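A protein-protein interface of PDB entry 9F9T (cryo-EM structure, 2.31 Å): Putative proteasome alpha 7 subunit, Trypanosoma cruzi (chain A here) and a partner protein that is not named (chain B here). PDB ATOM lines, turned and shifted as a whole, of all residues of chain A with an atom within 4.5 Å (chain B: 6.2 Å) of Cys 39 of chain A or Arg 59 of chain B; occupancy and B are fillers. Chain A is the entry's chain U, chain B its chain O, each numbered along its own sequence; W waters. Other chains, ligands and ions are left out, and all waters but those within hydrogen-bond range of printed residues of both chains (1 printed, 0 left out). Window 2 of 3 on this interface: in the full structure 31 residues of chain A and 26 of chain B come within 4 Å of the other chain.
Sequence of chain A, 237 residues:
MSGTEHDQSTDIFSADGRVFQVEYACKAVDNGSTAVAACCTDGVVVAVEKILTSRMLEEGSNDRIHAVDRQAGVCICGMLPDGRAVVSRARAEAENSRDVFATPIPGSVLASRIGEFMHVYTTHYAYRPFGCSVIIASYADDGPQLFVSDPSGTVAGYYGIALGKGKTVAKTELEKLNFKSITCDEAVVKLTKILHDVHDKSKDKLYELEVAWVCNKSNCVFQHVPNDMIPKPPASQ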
ATOM      1  N   ALA A  38      -4.317 -16.390 -14.103  1.00  0.00           N
ATOM      2  CA  ALA A  38      -3.694 -17.568 -13.507  1.00  0.00           C
ATOM      3  C   ALA A  38      -2.433 -17.189 -12.774  1.00  0.00           C
ATOM      4  O   ALA A  38      -1.579 -16.523 -13.362  1.00  0.00           O
ATOM      5  CB  ALA A  38      -3.315 -18.535 -14.569  1.00  0.00           C
ATOM      6  N   CYS A  39      -2.308 -17.619 -11.517  1.00  0.00           N
ATOM      7  CA  CYS A  39      -1.119 -17.355 -10.699  1.00  0.00           C
ATOM      8  C   CYS A  39      -0.243 -18.606 -10.719  1.00  0.00           C
ATOM      9  O   CYS A  39      -0.676 -19.676 -10.315  1.00  0.00           O
ATOM     10  CB  CYS A  39      -1.500 -17.008  -9.265  1.00  0.00           C
ATOM     11  SG  CYS A  39      -0.206 -16.197  -8.288  1.00  0.00           S
ATOM     12  N   CYS A  40       0.966 -18.461 -11.260  1.00  0.00           N
ATOM     13  CA  CYS A  40       1.782 -19.594 -11.653  1.00  0.00           C
ATOM     14  C   CYS A  40       2.990 -19.646 -10.725  1.00  0.00           C
ATOM     15  O   CYS A  40       3.053 -18.929  -9.735  1.00  0.00           O
ATOM     16  CB  CYS A  40       2.197 -19.448 -13.112  1.00  0.00           C
ATOM     17  SG  CYS A  40       0.816 -19.139 -14.256  1.00  0.00           S
ATOM     18  N   GLY A  43       5.189 -16.530 -12.030  1.00  0.00           N
ATOM     19  CA  GLY A  43       4.596 -15.230 -12.300  1.00  0.00           C
ATOM     20  C   GLY A  43       3.086 -15.283 -12.422  1.00  0.00           C
ATOM     21  O   GLY A  43       2.485 -16.315 -12.164  1.00  0.00           O
ATOM     22  N   VAL A  44       2.499 -14.219 -12.942  1.00  0.00           N
ATOM     23  CA  VAL A  44       1.071 -14.152 -13.166  1.00  0.00           C
ATOM     24  C   VAL A  44       0.819 -13.830 -14.623  1.00  0.00           C
ATOM     25  O   VAL A  44       1.466 -12.913 -15.137  1.00  0.00           O
ATOM     26  CB  VAL A  44       0.452 -13.039 -12.315  1.00  0.00           C
ATOM     27  CG1 VAL A  44      -1.055 -13.097 -12.379  1.00  0.00           C
ATOM     28  CG2 VAL A  44       0.890 -13.080 -10.871  1.00  0.00           C
ATOM     29  N   PRO A 144       4.525 -13.991  -6.616  1.00  0.00           N
ATOM     30  CA  PRO A 144       3.355 -13.869  -7.499  1.00  0.00           C
ATOM     31  C   PRO A 144       2.030 -13.730  -6.776  1.00  0.00           C
ATOM     32  O   PRO A 144       1.696 -14.555  -5.942  1.00  0.00           O
ATOM     33  CB  PRO A 144       3.292 -15.201  -8.258  1.00  0.00           C
ATOM     34  CG  PRO A 144       4.746 -15.657  -8.239  1.00  0.00           C
ATOM     35  CD  PRO A 144       5.325 -15.179  -6.914  1.00  0.00           C
ATOM     36  N   GLN A 145       1.277 -12.689  -7.074  1.00  0.00           N
ATOM     37  CA  GLN A 145      -0.025 -12.562  -6.447  1.00  0.00           C
ATOM     38  C   GLN A 145      -1.053 -12.129  -7.470  1.00  0.00           C
ATOM     39  O   GLN A 145      -0.791 -11.234  -8.248  1.00  0.00           O
ATOM     40  CB  GLN A 145      -0.052 -11.463  -5.403  1.00  0.00           C
ATOM     41  CG  GLN A 145       1.018 -11.557  -4.320  1.00  0.00           C
ATOM     42  CD  GLN A 145       0.644 -12.521  -3.230  1.00  0.00           C
ATOM     43  OE1 GLN A 145      -0.490 -12.560  -2.749  1.00  0.00           O
ATOM     44  NE2 GLN A 145       1.592 -13.378  -2.907  1.00  0.00           N
ATOM     45  N   LEU A 146      -2.248 -12.662  -7.346  1.00  0.00           N
ATOM     46  CA  LEU A 146      -3.405 -12.313  -8.142  1.00  0.00           C
ATOM     47  C   LEU A 146      -4.588 -12.012  -7.240  1.00  0.00           C
ATOM     48  O   LEU A 146      -5.086 -12.902  -6.554  1.00  0.00           O
ATOM     49  CB  LEU A 146      -3.673 -13.545  -8.965  1.00  0.00           C
ATOM     50  CG  LEU A 146      -4.932 -13.480  -9.772  1.00  0.00           C
ATOM     51  CD1 LEU A 146      -4.904 -12.313 -10.756  1.00  0.00           C
ATOM     52  CD2 LEU A 146      -5.111 -14.776 -10.501  1.00  0.00           C
ATOM     53  N   GLY A 157      -7.836 -12.975  -2.859  1.00  0.00           N
ATOM     54  CA  GLY A 157      -6.745 -13.553  -3.618  1.00  0.00           C
ATOM     55  C   GLY A 157      -7.131 -14.896  -4.220  1.00  0.00           C
ATOM     56  O   GLY A 157      -7.939 -15.635  -3.701  1.00  0.00           O
ATOM     57  N   TYR A 158      -6.500 -15.176  -5.336  1.00  0.00           N
ATOM     58  CA  TYR A 158      -6.889 -16.281  -6.165  1.00  0.00           C
ATOM     59  C   TYR A 158      -5.702 -17.030  -6.741  1.00  0.00           C
ATOM     60  O   TYR A 158      -4.733 -16.424  -7.091  1.00  0.00           O
ATOM     61  CB  TYR A 158      -7.662 -15.663  -7.331  1.00  0.00           C
ATOM     62  CG  TYR A 158      -9.086 -15.321  -7.027  1.00  0.00           C
ATOM     63  CD1 TYR A 158     -10.061 -16.304  -7.030  1.00  0.00           C
ATOM     64  CD2 TYR A 158      -9.439 -14.037  -6.712  1.00  0.00           C
ATOM     65  CE1 TYR A 158     -11.360 -16.006  -6.658  1.00  0.00           C
ATOM     66  CE2 TYR A 158     -10.739 -13.717  -6.391  1.00  0.00           C
ATOM     67  CZ  TYR A 158     -11.686 -14.707  -6.347  1.00  0.00           C
ATOM     68  OH  TYR A 158     -12.959 -14.336  -6.072  1.00  0.00           O
ATOM     69  N   TYR A 159      -5.884 -18.287  -7.059  1.00  0.00           N
ATOM     70  CA  TYR A 159      -4.939 -18.975  -7.922  1.00  0.00           C
ATOM     71  C   TYR A 159      -5.261 -18.742  -9.379  1.00  0.00           C
ATOM     72  O   TYR A 159      -4.378 -18.665 -10.182  1.00  0.00           O
ATOM     73  CB  TYR A 159      -4.993 -20.501  -7.740  1.00  0.00           C
ATOM     74  CG  TYR A 159      -4.492 -20.935  -6.361  1.00  0.00           C
ATOM     75  CD1 TYR A 159      -3.173 -20.771  -5.955  1.00  0.00           C
ATOM     76  CD2 TYR A 159      -5.377 -21.475  -5.442  1.00  0.00           C
ATOM     77  CE1 TYR A 159      -2.755 -21.164  -4.685  1.00  0.00           C
ATOM     78  CE2 TYR A 159      -4.977 -21.892  -4.188  1.00  0.00           C
ATOM     79  CZ  TYR A 159      -3.667 -21.727  -3.798  1.00  0.00           C
ATOM     80  OH  TYR A 159      -3.402 -22.172  -2.525  1.00  0.00           O
ATOM     81  N   PHE A 179      -2.135 -25.866 -10.506  1.00  0.00           N
ATOM     82  CA  PHE A 179      -1.615 -24.550 -10.178  1.00  0.00           C
ATOM     83  C   PHE A 179      -0.288 -24.651  -9.428  1.00  0.00           C
ATOM     84  O   PHE A 179       0.401 -23.642  -9.249  1.00  0.00           O
ATOM     85  CB  PHE A 179      -2.695 -23.733  -9.451  1.00  0.00           C
ATOM     86  CG  PHE A 179      -3.771 -23.206 -10.368  1.00  0.00           C
ATOM     87  CD1 PHE A 179      -3.562 -22.081 -11.140  1.00  0.00           C
ATOM     88  CD2 PHE A 179      -4.977 -23.861 -10.495  1.00  0.00           C
ATOM     89  CE1 PHE A 179      -4.549 -21.594 -11.997  1.00  0.00           C
ATOM     90  CE2 PHE A 179      -5.966 -23.395 -11.350  1.00  0.00           C
ATOM     91  CZ  PHE A 179      -5.744 -22.270 -12.118  1.00  0.00           C
ATOM     92  N   VAL B  53     -14.303 -20.552   2.236  1.00  0.00           N
ATOM     93  CA  VAL B  53     -13.696 -20.478   0.926  1.00  0.00           C
ATOM     94  C   VAL B  53     -14.580 -21.320   0.006  1.00  0.00           C
ATOM     95  O   VAL B  53     -14.287 -22.485  -0.250  1.00  0.00           O
ATOM     96  CB  VAL B  53     -12.230 -20.959   0.977  1.00  0.00           C
ATOM     97  CG1 VAL B  53     -11.548 -20.930  -0.388  1.00  0.00           C
ATOM     98  CG2 VAL B  53     -11.411 -20.151   1.982  1.00  0.00           C
ATOM     99  N   ASP B  55     -15.125 -21.189  -3.202  1.00  0.00           N
ATOM    100  CA  ASP B  55     -14.476 -21.313  -4.503  1.00  0.00           C
ATOM    101  C   ASP B  55     -13.164 -22.108  -4.405  1.00  0.00           C
ATOM    102  O   ASP B  55     -12.233 -21.739  -3.696  1.00  0.00           O
ATOM    103  CB  ASP B  55     -14.210 -19.884  -5.011  1.00  0.00           C
ATOM    104  CG  ASP B  55     -14.006 -19.699  -6.506  1.00  0.00           C
ATOM    105  OD1 ASP B  55     -13.909 -20.725  -7.235  1.00  0.00           O
ATOM    106  OD2 ASP B  55     -13.958 -18.518  -6.935  1.00  0.00           O
ATOM    107  N   LEU B  57     -10.784 -22.156  -6.315  1.00  0.00           N
ATOM    108  CA  LEU B  57      -9.685 -21.413  -6.913  1.00  0.00           C
ATOM    109  C   LEU B  57      -9.200 -20.232  -6.075  1.00  0.00           C
ATOM    110  O   LEU B  57      -8.268 -19.543  -6.489  1.00  0.00           O
ATOM    111  CB  LEU B  57     -10.189 -20.863  -8.239  1.00  0.00           C
ATOM    112  CG  LEU B  57      -9.709 -21.517  -9.538  1.00  0.00           C
ATOM    113  CD1 LEU B  57      -9.487 -23.009  -9.414  1.00  0.00           C
ATOM    114  CD2 LEU B  57     -10.743 -21.216 -10.608  1.00  0.00           C
ATOM    115  N   MET B  58      -9.831 -19.953  -4.928  1.00  0.00           N
ATOM    116  CA  MET B  58      -9.383 -18.878  -4.064  1.00  0.00           C
ATOM    117  C   MET B  58      -8.172 -19.309  -3.238  1.00  0.00           C
ATOM    118  O   MET B  58      -8.082 -20.435  -2.792  1.00  0.00           O
ATOM    119  CB  MET B  58     -10.485 -18.517  -3.086  1.00  0.00           C
ATOM    120  CG  MET B  58     -11.213 -17.259  -3.398  1.00  0.00           C
ATOM    121  SD  MET B  58     -12.579 -17.005  -2.209  1.00  0.00           S
ATOM    122  CE  MET B  58     -13.749 -16.133  -3.250  1.00  0.00           C
ATOM    123  N   ARG B  59      -7.280 -18.363  -2.988  1.00  0.00           N
ATOM    124  CA  ARG B  59      -6.094 -18.536  -2.184  1.00  0.00           C
ATOM    125  C   ARG B  59      -6.564 -18.402  -0.747  1.00  0.00           C
ATOM    126  O   ARG B  59      -6.931 -17.307  -0.318  1.00  0.00           O
ATOM    127  CB  ARG B  59      -5.053 -17.486  -2.579  1.00  0.00           C
ATOM    128  CG  ARG B  59      -3.628 -17.991  -2.736  1.00  0.00           C
ATOM    129  CD  ARG B  59      -2.604 -16.899  -2.491  1.00  0.00           C
ATOM    130  NE  ARG B  59      -1.228 -17.364  -2.469  1.00  0.00           N
ATOM    131  CZ  ARG B  59      -0.352 -17.251  -3.472  1.00  0.00           C
ATOM    132  NH1 ARG B  59       0.892 -17.658  -3.290  1.00  0.00           N
ATOM    133  NH2 ARG B  59      -0.700 -16.764  -4.655  1.00  0.00           N
ATOM    134  N   PRO B  60      -6.717 -19.524   0.004  1.00  0.00           N
ATOM    135  CA  PRO B  60      -7.436 -19.473   1.284  1.00  0.00           C
ATOM    136  C   PRO B  60      -6.698 -18.649   2.347  1.00  0.00           C
ATOM    137  O   PRO B  60      -7.328 -17.971   3.149  1.00  0.00           O
ATOM    138  CB  PRO B  60      -7.727 -20.964   1.549  1.00  0.00           C
ATOM    139  CG  PRO B  60      -6.598 -21.708   0.858  1.00  0.00           C
ATOM    140  CD  PRO B  60      -6.289 -20.893  -0.373  1.00  0.00           C
ATOM    141  N   ASP B  61      -5.381 -18.501   2.286  1.00  0.00           N
ATOM    142  CA  ASP B  61      -4.718 -17.615   3.251  1.00  0.00           C
ATOM    143  C   ASP B  61      -4.938 -16.124   2.996  1.00  0.00           C
ATOM    144  O   ASP B  61      -4.181 -15.311   3.507  1.00  0.00           O
ATOM    145  CB  ASP B  61      -3.201 -17.809   3.256  1.00  0.00           C
ATOM    146  CG  ASP B  61      -2.595 -17.658   1.875  1.00  0.00           C
ATOM    147  OD1 ASP B  61      -1.923 -16.622   1.632  1.00  0.00           O
ATOM    148  OD2 ASP B  61      -2.813 -18.582   1.041  1.00  0.00           O
ATOM    149  N   THR B  62      -5.887 -15.730   2.151  1.00  0.00           N
ATOM    150  CA  THR B  62      -6.112 -14.324   1.881  1.00  0.00           C
ATOM    151  C   THR B  62      -7.502 -13.951   2.364  1.00  0.00           C
ATOM    152  O   THR B  62      -7.874 -12.796   2.323  1.00  0.00           O
ATOM    153  CB  THR B  62      -5.953 -13.949   0.389  1.00  0.00           C
ATOM    154  OG1 THR B  62      -6.935 -14.594  -0.428  1.00  0.00           O
ATOM    155  CG2 THR B  62      -4.589 -14.277  -0.186  1.00  0.00           C
ATOM    156  N   ILE B  63      -8.318 -14.948   2.661  1.00  0.00           N
ATOM    157  CA  ILE B  63      -9.644 -14.720   3.184  1.00  0.00           C
ATOM    158  C   ILE B  63      -9.518 -14.726   4.695  1.00  0.00           C
ATOM    159  O   ILE B  63      -9.123 -15.728   5.295  1.00  0.00           O
ATOM    160  CB  ILE B  63     -10.631 -15.800   2.727  1.00  0.00           C
ATOM    161  CG1 ILE B  63     -10.524 -16.073   1.223  1.00  0.00           C
ATOM    162  CG2 ILE B  63     -12.034 -15.413   3.161  1.00  0.00           C
ATOM    163  CD1 ILE B  63     -10.361 -14.822   0.375  1.00  0.00           C
HETATM  164  O   HOH W   1       1.627 -15.648  -0.784  1.00  0.00           O
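Hydrophobic or aromatic side chains of chain A within 4 Å of the printed part of chain B: Tyr 158 and Tyr 159. Of the 9 printed residues of chain B, 6 touch a printed residue of chain A. Hydrophobic or aromatic side chains of chain B that line the printed part of chain A: Met 58 and Pro 60. Among the printed residues, 13 pairs touch across the chains.
Cys 39 of chain A touches one residue of chain B. Of the printed residues of chain B, Gly 157 of chain A touches Met 58 (3.6 Å), Arg 59 (2.9 Å) and Thr 62 (3.1 Å). Printed residues of chain A within 4 Å of Leu 57 of chain B: Tyr 158 and Tyr 159. Printed residues of chain A within 4 Å of Met 58 of chain B: Gly 157 (3.6 Å), Tyr 158 (3.4 Å) and Tyr 159 (3.7 Å). The nearest printed residue of chain B that does not touch Cys 39 of chain A is Leu 57 of chain B (7.7 Å). The nearest residue of chain A that does not touch Arg 59 of chain B is Gln 145 of chain A (4.4 Å).
Water W1 bridges NE2 of Gln 145 of chain A (3.1 Å) and NH1 of Arg 59 of chain B (3.3 Å).
The backbone carbonyl oxygen of Leu 57 of chain B sits at hydrogen-bond distance from the backbone NH of Tyr 159 of chain A (2.8 Å). The guanidinium group of Arg 59 of chain B sits at hydrogen-bond distance from the side-chain sulfur of Cys 39 of chain A (3.7 Å). The backbone NH (N) of Arg 59 of chain B sits at hydrogen-bond distance from the backbone carbonyl oxygen (O) of Gly 157 of chain A, at 2.9 Å. The side-chain hydroxyl (OG1) of Thr 62 of chain B lies within hydrogen-bond range of the backbone NH (N) of Gly 157 of chain A.
Among the printed residues, merely in contact across the chains: Pro 144 of chain A with Arg 59 of chain B, Gly 157 of chain A with Met 58 of chain B, Tyr 158 of chain A with Asp 55 of chain B, Tyr 158 of chain A with Leu 57 of chain B, Tyr 158 of chain A with Met 58 of chain B, Tyr 158 of chain A with Arg 59 of chain B, Tyr 159 of chain A with Met 58 of chain B, Tyr 159 of chain A with Arg 59 of chain B and Tyr 159 of chain A with Pro 60 of chain B.
OG1 of Thr 62 of chain B lies within hydrogen-bond range of O of Arg 59 of chain B (2.7 Å). SG of Cys 39 of chain A is in hydrogen-bond range of O of Pro 144 of chain A (3.4 Å). O of Tyr 159 of chain A lies within hydrogen-bond range of N of Cys 39 of chain A. O of Leu 146 of chain A is in hydrogen-bond range of N of Tyr 158 of chain A, 2.9 Å away.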
